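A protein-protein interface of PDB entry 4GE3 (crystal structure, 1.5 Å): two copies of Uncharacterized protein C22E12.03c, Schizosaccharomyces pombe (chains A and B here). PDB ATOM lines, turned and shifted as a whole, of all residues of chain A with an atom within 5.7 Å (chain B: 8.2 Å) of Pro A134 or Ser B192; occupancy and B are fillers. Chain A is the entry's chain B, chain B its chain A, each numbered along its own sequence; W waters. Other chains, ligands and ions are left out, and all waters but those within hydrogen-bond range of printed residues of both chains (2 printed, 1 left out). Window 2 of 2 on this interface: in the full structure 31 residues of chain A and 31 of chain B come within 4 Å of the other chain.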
ATOM      1  N   GLY A 132     -29.181  -6.312 -34.791  1.00  0.00           N
ATOM      2  CA  GLY A 132     -30.177  -5.413 -34.227  1.00  0.00           C
ATOM      3  C   GLY A 132     -29.549  -4.796 -33.014  1.00  0.00           C
ATOM      4  O   GLY A 132     -28.353  -4.950 -32.775  1.00  0.00           O
ATOM      5  N   HIS A 133     -30.357  -4.091 -32.244  1.00  0.00           N
ATOM      6  CA  HIS A 133     -29.831  -3.520 -31.035  1.00  0.00           C
ATOM      7  C   HIS A 133     -29.518  -4.630 -30.072  1.00  0.00           C
ATOM      8  O   HIS A 133     -30.298  -5.575 -29.964  1.00  0.00           O
ATOM      9  CB  HIS A 133     -30.796  -2.517 -30.420  1.00  0.00           C
ATOM     10  CG  HIS A 133     -30.126  -1.598 -29.442  1.00  0.00           C
ATOM     11  ND1 HIS A 133     -30.142  -1.810 -28.084  1.00  0.00           N
ATOM     12  CD2 HIS A 133     -29.392  -0.475 -29.640  1.00  0.00           C
ATOM     13  CE1 HIS A 133     -29.457  -0.850 -27.481  1.00  0.00           C
ATOM     14  NE2 HIS A 133     -28.985  -0.032 -28.404  1.00  0.00           N
ATOM     15  N   PRO A 134     -28.351  -4.558 -29.411  1.00  0.00           N
ATOM     16  CA  PRO A 134     -28.044  -5.575 -28.400  1.00  0.00           C
ATOM     17  C   PRO A 134     -29.229  -5.850 -27.457  1.00  0.00           C
ATOM     18  O   PRO A 134     -29.367  -6.975 -26.986  1.00  0.00           O
ATOM     19  CB  PRO A 134     -26.846  -4.974 -27.658  1.00  0.00           C
ATOM     20  CG  PRO A 134     -26.116  -4.193 -28.771  1.00  0.00           C
ATOM     21  CD  PRO A 134     -27.176  -3.728 -29.744  1.00  0.00           C
ATOM     22  N   SER A 135     -30.105  -4.868 -27.228  1.00  0.00           N
ATOM     23  CA  SER A 135     -31.264  -5.089 -26.334  1.00  0.00           C
ATOM     24  C   SER A 135     -32.333  -6.032 -26.908  1.00  0.00           C
ATOM     25  O   SER A 135     -33.172  -6.529 -26.162  1.00  0.00           O
ATOM     26  CB  SER A 135     -31.921  -3.762 -25.948  1.00  0.00           C
ATOM     27  OG  SER A 135     -32.470  -3.140 -27.095  1.00  0.00           O
ATOM     28  N   VAL A 136     -32.310  -6.269 -28.218  1.00  0.00           N
ATOM     29  CA  VAL A 136     -33.237  -7.236 -28.820  1.00  0.00           C
ATOM     30  C   VAL A 136     -32.543  -8.530 -29.273  1.00  0.00           C
ATOM     31  O   VAL A 136     -33.165  -9.371 -29.933  1.00  0.00           O
ATOM     32  CB  VAL A 136     -34.130  -6.622 -29.982  1.00  0.00           C
ATOM     33  CG1 VAL A 136     -35.012  -5.465 -29.471  1.00  0.00           C
ATOM     34  CG2 VAL A 136     -33.293  -6.204 -31.190  1.00  0.00           C
ATOM     35  N   ARG A 137     -31.272  -8.700 -28.890  1.00  0.00           N
ATOM     36  CA  ARG A 137     -30.477  -9.856 -29.302  1.00  0.00           C
ATOM     37  C   ARG A 137     -31.142 -11.172 -28.879  1.00  0.00           C
ATOM     38  O   ARG A 137     -31.311 -12.083 -29.701  1.00  0.00           O
ATOM     39  CB  ARG A 137     -29.050  -9.777 -28.742  1.00  0.00           C
ATOM     40  CG  ARG A 137     -28.113 -10.825 -29.320  1.00  0.00           C
ATOM     41  CD  ARG A 137     -26.855 -11.003 -28.487  1.00  0.00           C
ATOM     42  NE  ARG A 137     -25.990 -12.044 -29.041  1.00  0.00           N
ATOM     43  CZ  ARG A 137     -24.742 -11.852 -29.466  1.00  0.00           C
ATOM     44  NH1 ARG A 137     -24.182 -10.649 -29.406  1.00  0.00           N
ATOM     45  NH2 ARG A 137     -24.051 -12.867 -29.960  1.00  0.00           N
ATOM     46  N   GLY A 138     -31.526 -11.248 -27.603  1.00  0.00           N
ATOM     47  CA  GLY A 138     -32.198 -12.432 -27.042  1.00  0.00           C
ATOM     48  C   GLY A 138     -33.440 -12.788 -27.835  1.00  0.00           C
ATOM     49  O   GLY A 138     -33.631 -13.942 -28.238  1.00  0.00           O
ATOM     50  N   TYR A 147     -27.293 -13.967 -34.756  1.00  0.00           N
ATOM     51  CA  TYR A 147     -26.971 -12.548 -34.541  1.00  0.00           C
ATOM     52  C   TYR A 147     -25.489 -12.278 -34.805  1.00  0.00           C
ATOM     53  O   TYR A 147     -24.611 -12.936 -34.225  1.00  0.00           O
ATOM     54  CB  TYR A 147     -27.337 -12.133 -33.105  1.00  0.00           C
ATOM     55  CG  TYR A 147     -27.060 -10.688 -32.763  1.00  0.00           C
ATOM     56  CD1 TYR A 147     -25.774 -10.260 -32.402  1.00  0.00           C
ATOM     57  CD2 TYR A 147     -28.090  -9.749 -32.781  1.00  0.00           C
ATOM     58  CE1 TYR A 147     -25.523  -8.919 -32.092  1.00  0.00           C
ATOM     59  CE2 TYR A 147     -27.844  -8.410 -32.455  1.00  0.00           C
ATOM     60  CZ  TYR A 147     -26.557  -8.018 -32.114  1.00  0.00           C
ATOM     61  OH  TYR A 147     -26.351  -6.698 -31.810  1.00  0.00           O
ATOM     62  N   GLN A 162     -27.802  -2.010 -36.217  1.00  0.00           N
ATOM     63  CA  GLN A 162     -27.835  -2.044 -34.752  1.00  0.00           C
ATOM     64  C   GLN A 162     -28.510  -0.912 -33.971  1.00  0.00           C
ATOM     65  O   GLN A 162     -29.282  -1.179 -33.039  1.00  0.00           O
ATOM     66  CB  GLN A 162     -26.426  -2.224 -34.210  1.00  0.00           C
ATOM     67  CG  GLN A 162     -25.792  -3.540 -34.638  1.00  0.00           C
ATOM     68  CD  GLN A 162     -24.468  -3.803 -33.954  1.00  0.00           C
ATOM     69  OE1 GLN A 162     -23.557  -2.966 -34.004  1.00  0.00           O
ATOM     70  NE2 GLN A 162     -24.351  -4.964 -33.300  1.00  0.00           N
ATOM     71  N   GLY A 163     -28.201   0.342 -34.290  1.00  0.00           N
ATOM     72  CA  GLY A 163     -28.647   1.402 -33.389  1.00  0.00           C
ATOM     73  C   GLY A 163     -28.395   2.769 -33.958  1.00  0.00           C
ATOM     74  O   GLY A 163     -28.051   2.900 -35.140  1.00  0.00           O
ATOM     75  N   PRO A 164     -28.555   3.800 -33.117  1.00  0.00           N
ATOM     76  CA  PRO A 164     -28.425   5.167 -33.664  1.00  0.00           C
ATOM     77  C   PRO A 164     -27.035   5.384 -34.218  1.00  0.00           C
ATOM     78  O   PRO A 164     -26.894   6.057 -35.244  1.00  0.00           O
ATOM     79  CB  PRO A 164     -28.668   6.075 -32.445  1.00  0.00           C
ATOM     80  CG  PRO A 164     -29.199   5.195 -31.367  1.00  0.00           C
ATOM     81  CD  PRO A 164     -29.004   3.773 -31.709  1.00  0.00           C
ATOM     82  N   GLY A 165     -26.009   4.826 -33.565  1.00  0.00           N
ATOM     83  CA  GLY A 165     -24.645   4.978 -34.069  1.00  0.00           C
ATOM     84  C   GLY A 165     -24.369   4.372 -35.425  1.00  0.00           C
ATOM     85  O   GLY A 165     -23.388   4.730 -36.065  1.00  0.00           O
ATOM     86  N   THR A 166     -25.231   3.458 -35.879  1.00  0.00           N
ATOM     87  CA  THR A 166     -25.026   2.809 -37.180  1.00  0.00           C
ATOM     88  C   THR A 166     -26.040   3.279 -38.221  1.00  0.00           C
ATOM     89  O   THR A 166     -26.100   2.699 -39.326  1.00  0.00           O
ATOM     90  CB  THR A 166     -25.061   1.258 -37.057  1.00  0.00           C
ATOM     91  OG1 THR A 166     -26.396   0.847 -36.680  1.00  0.00           O
ATOM     92  CG2 THR A 166     -24.045   0.776 -36.010  1.00  0.00           C
ATOM     93  N   ARG B  29     -31.020  11.222 -24.357  1.00  0.00           N
ATOM     94  CA  ARG B  29     -30.615   9.970 -23.708  1.00  0.00           C
ATOM     95  C   ARG B  29     -29.890  10.214 -22.386  1.00  0.00           C
ATOM     96  O   ARG B  29     -30.025   9.429 -21.438  1.00  0.00           O
ATOM     97  CB  ARG B  29     -29.736   9.146 -24.646  1.00  0.00           C
ATOM     98  CG  ARG B  29     -30.567   8.430 -25.691  1.00  0.00           C
ATOM     99  CD  ARG B  29     -29.682   7.944 -26.801  1.00  0.00           C
ATOM    100  NE  ARG B  29     -30.372   7.116 -27.777  1.00  0.00           N
ATOM    101  CZ  ARG B  29     -31.102   7.619 -28.776  1.00  0.00           C
ATOM    102  NH1 ARG B  29     -31.266   8.931 -28.916  1.00  0.00           N
ATOM    103  NH2 ARG B  29     -31.660   6.785 -29.640  1.00  0.00           N
ATOM    104  N   MET B 168     -22.865  12.203 -34.964  1.00  0.00           N
ATOM    105  CA  MET B 168     -22.863  11.443 -33.722  1.00  0.00           C
ATOM    106  C   MET B 168     -21.586  11.653 -32.888  1.00  0.00           C
ATOM    107  O   MET B 168     -21.664  11.912 -31.683  1.00  0.00           O
ATOM    108  CB  MET B 168     -23.055   9.944 -33.978  1.00  0.00           C
ATOM    109  CG  MET B 168     -24.420   9.594 -34.502  1.00  0.00           C
ATOM    110  SD  MET B 168     -25.807   9.885 -33.364  1.00  0.00           S
ATOM    111  CE  MET B 168     -25.513   8.587 -32.175  1.00  0.00           C
ATOM    112  N   ALA B 186     -22.376   5.104 -20.311  1.00  0.00           N
ATOM    113  CA  ALA B 186     -23.685   4.445 -20.452  1.00  0.00           C
ATOM    114  C   ALA B 186     -24.427   4.917 -21.710  1.00  0.00           C
ATOM    115  O   ALA B 186     -24.978   4.097 -22.479  1.00  0.00           O
ATOM    116  CB  ALA B 186     -24.543   4.670 -19.198  1.00  0.00           C
ATOM    117  N   VAL B 187     -24.425   6.227 -21.933  1.00  0.00           N
ATOM    118  CA  VAL B 187     -25.045   6.764 -23.138  1.00  0.00           C
ATOM    119  C   VAL B 187     -24.317   6.240 -24.373  1.00  0.00           C
ATOM    120  O   VAL B 187     -24.952   5.755 -25.317  1.00  0.00           O
ATOM    121  CB  VAL B 187     -25.106   8.277 -23.143  1.00  0.00           C
ATOM    122  CG1 VAL B 187     -25.578   8.759 -24.509  1.00  0.00           C
ATOM    123  CG2 VAL B 187     -26.063   8.748 -22.026  1.00  0.00           C
ATOM    124  N   TYR B 188     -22.990   6.300 -24.340  1.00  0.00           N
ATOM    125  CA  TYR B 188     -22.213   5.834 -25.471  1.00  0.00           C
ATOM    126  C   TYR B 188     -22.548   4.385 -25.812  1.00  0.00           C
ATOM    127  O   TYR B 188     -22.810   4.027 -26.973  1.00  0.00           O
ATOM    128  CB  TYR B 188     -20.722   5.980 -25.159  1.00  0.00           C
ATOM    129  CG  TYR B 188     -19.830   5.593 -26.318  1.00  0.00           C
ATOM    130  CD1 TYR B 188     -19.505   4.263 -26.542  1.00  0.00           C
ATOM    131  CD2 TYR B 188     -19.295   6.562 -27.168  1.00  0.00           C
ATOM    132  CE1 TYR B 188     -18.672   3.887 -27.589  1.00  0.00           C
ATOM    133  CE2 TYR B 188     -18.450   6.187 -28.237  1.00  0.00           C
ATOM    134  CZ  TYR B 188     -18.164   4.857 -28.437  1.00  0.00           C
ATOM    135  OH  TYR B 188     -17.347   4.428 -29.473  1.00  0.00           O
ATOM    136  N   LYS B 189     -22.569   3.544 -24.788  1.00  0.00           N
ATOM    137  CA  LYS B 189     -22.821   2.130 -24.974  1.00  0.00           C
ATOM    138  C   LYS B 189     -24.166   1.886 -25.625  1.00  0.00           C
ATOM    139  O   LYS B 189     -24.286   1.003 -26.499  1.00  0.00           O
ATOM    140  CB  LYS B 189     -22.749   1.401 -23.637  1.00  0.00           C
ATOM    141  CG  LYS B 189     -22.818  -0.107 -23.767  1.00  0.00           C
ATOM    142  CD  LYS B 189     -22.679  -0.776 -22.418  1.00  0.00           C
ATOM    143  CE  LYS B 189     -22.712  -2.307 -22.527  1.00  0.00           C
ATOM    144  NZ  LYS B 189     -22.781  -2.973 -21.191  1.00  0.00           N
ATOM    145  N   SER B 190     -25.166   2.682 -25.233  1.00  0.00           N
ATOM    146  CA  SER B 190     -26.536   2.507 -25.732  1.00  0.00           C
ATOM    147  C   SER B 190     -26.683   2.835 -27.226  1.00  0.00           C
ATOM    148  O   SER B 190     -27.712   2.506 -27.827  1.00  0.00           O
ATOM    149  CB  SER B 190     -27.521   3.410 -24.968  1.00  0.00           C
ATOM    150  OG  SER B 190     -27.369   4.782 -25.282  1.00  0.00           O
ATOM    151  N   LEU B 191     -25.699   3.533 -27.799  1.00  0.00           N
ATOM    152  CA  LEU B 191     -25.811   4.005 -29.194  1.00  0.00           C
ATOM    153  C   LEU B 191     -25.365   2.983 -30.244  1.00  0.00           C
ATOM    154  O   LEU B 191     -25.675   3.140 -31.426  1.00  0.00           O
ATOM    155  CB  LEU B 191     -25.019   5.292 -29.402  1.00  0.00           C
ATOM    156  CG  LEU B 191     -25.374   6.459 -28.507  1.00  0.00           C
ATOM    157  CD1 LEU B 191     -24.389   7.616 -28.761  1.00  0.00           C
ATOM    158  CD2 LEU B 191     -26.803   6.921 -28.762  1.00  0.00           C
ATOM    159  N   SER B 192     -24.660   1.931 -29.829  1.00  0.00           N
ATOM    160  CA  SER B 192     -24.061   0.974 -30.751  1.00  0.00           C
ATOM    161  C   SER B 192     -23.149   1.689 -31.751  1.00  0.00           C
ATOM    162  O   SER B 192     -23.301   1.525 -32.959  1.00  0.00           O
ATOM    163  CB  SER B 192     -25.129   0.153 -31.478  1.00  0.00           C
ATOM    164  OG  SER B 192     -25.522  -0.942 -30.703  1.00  0.00           O
ATOM    165  N   MET B 193     -22.196   2.481 -31.243  1.00  0.00           N
ATOM    166  CA  MET B 193     -21.243   3.177 -32.114  1.00  0.00           C
ATOM    167  C   MET B 193     -20.399   2.112 -32.831  1.00  0.00           C
ATOM    168  O   MET B 193     -20.018   1.088 -32.222  1.00  0.00           O
ATOM    169  CB  MET B 193     -20.340   4.095 -31.290  1.00  0.00           C
ATOM    170  CG  MET B 193     -21.086   5.246 -30.636  1.00  0.00           C
ATOM    171  SD  MET B 193     -21.861   6.344 -31.874  1.00  0.00           S
ATOM    172  CE  MET B 193     -20.385   7.190 -32.499  1.00  0.00           C
ATOM    173  N   PRO B 194     -20.104   2.318 -34.127  1.00  0.00           N
ATOM    174  CA  PRO B 194     -19.356   1.274 -34.856  1.00  0.00           C
ATOM    175  C   PRO B 194     -17.895   1.206 -34.453  1.00  0.00           C
ATOM    176  O   PRO B 194     -17.332   2.207 -34.035  1.00  0.00           O
ATOM    177  CB  PRO B 194     -19.495   1.689 -36.322  1.00  0.00           C
ATOM    178  CG  PRO B 194     -19.863   3.136 -36.298  1.00  0.00           C
ATOM    179  CD  PRO B 194     -20.566   3.412 -35.003  1.00  0.00           C
ATOM    180  OXT PRO B 194     -17.279   0.135 -34.539  1.00  0.00           O
HETATM  181  O   HOH W   1     -26.009  -0.601 -27.899  1.00  0.00           O
HETATM  182  O   HOH W   2     -22.124   7.097 -35.455  1.00  0.00           O
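No position is printed for both chains.
Printed residues of chain A that touch a printed residue of chain B: His A133, Pro A134, Gln A162, Gly A163, Pro A164, Gly A165 and Thr A166.
Hydrophobic or aromatic side chains of chain A that line the printed part of chain B: His A133, Pro A134 and Pro A164.
Hydrophobic or aromatic side chains of chain B within 4 Å of the printed part of chain A: Leu B191, Met B193 and Pro B194.
Among the printed residues, 11 pairs touch across the chains.
Among the printed residues, no Asp or Glu carboxylate lies within 4 Å of a Lys or Arg side-chain nitrogen of the other chain.
OG of Ser B192 touches CD of Pro A134 (3.4 Å).
Gln A162 touches Ser B192 (CB to OG, 3.8 Å).
Gly A163 touches Leu B191 (C to O, 3.7 Å).
Arg B29 touches Pro A164.
O of Ser B192 touches CA of Gly A165 (3.9 Å).
SD of Met B193 touches CA of Gly A165 (3.8 Å).
Gly A165 touches Pro B194.
Thr A166 touches Ser B192.
Pro A134 touches just one residue of chain B: Ser B192 (3.4 Å).
Ser B192 touches four residues of chain A.
Printed residues of chain B within 4 Å of Gly A165: Leu B191 (2.7 Å), Ser B192 (3.9 Å), Met B193 (3.8 Å) and Pro B194 (3.3 Å).
Of the printed residues of chain B, Gln A162 touches Ser B192 (3.8 Å).
Printed residues of chain A within 4 Å of Met B193: Gly A165.
Of the printed residues of chain A, Pro B194 touches Gly A165 (3.3 Å).
Of the printed residues of chain A, Arg B29 touches Pro A164.
Ala B186 touches none of the printed residues of chain A.
Val B187 touches none of the printed residues of chain A.
The nearest residue of chain A that does not touch Ser B192 is His A133 (4.04 Å).
N of Gly A163 is in hydrogen-bond range of OG1 of Thr A166 (3.0 Å).
The backbone carbonyl oxygen (O) of Gln A162 lies close to the backbone NH (N) of His A133 (3.2 Å).
The side-chain hydroxyl (OG) of Ser A135 sits at hydrogen-bond distance from a ring nitrogen (ND1) of His A133.
O of Val B187 is in hydrogen-bond range of OG of Ser B190, 2.6 Å away.
The side-chain hydroxyl (OH) of Tyr A147 sits at hydrogen-bond distance from the side-chain amide nitrogen (NE2) of Gln A162 (3.0 Å).
The backbone NH (N) of Gln A162 is in hydrogen-bond range of the side-chain hydroxyl (OG1) of Thr A166 (3.2 Å).
O of Leu B191 is in hydrogen-bond range of N of Gly A165 (2.7 Å).
O of Leu B191 sits close to N of Pro A164 (3.4 Å).
NE2 of His A133 sits at hydrogen-bond distance from O of Ser B190 (2.9 Å).
Water W1 lies within hydrogen-bond range of the backbone carbonyl oxygen of Lys B189, the side-chain hydroxyl of Ser B192 and a ring nitrogen (NE2) of His A133.
Water W2 bridges the backbone carbonyl oxygen of Gly A165 and the side-chain sulfur of Met B193.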
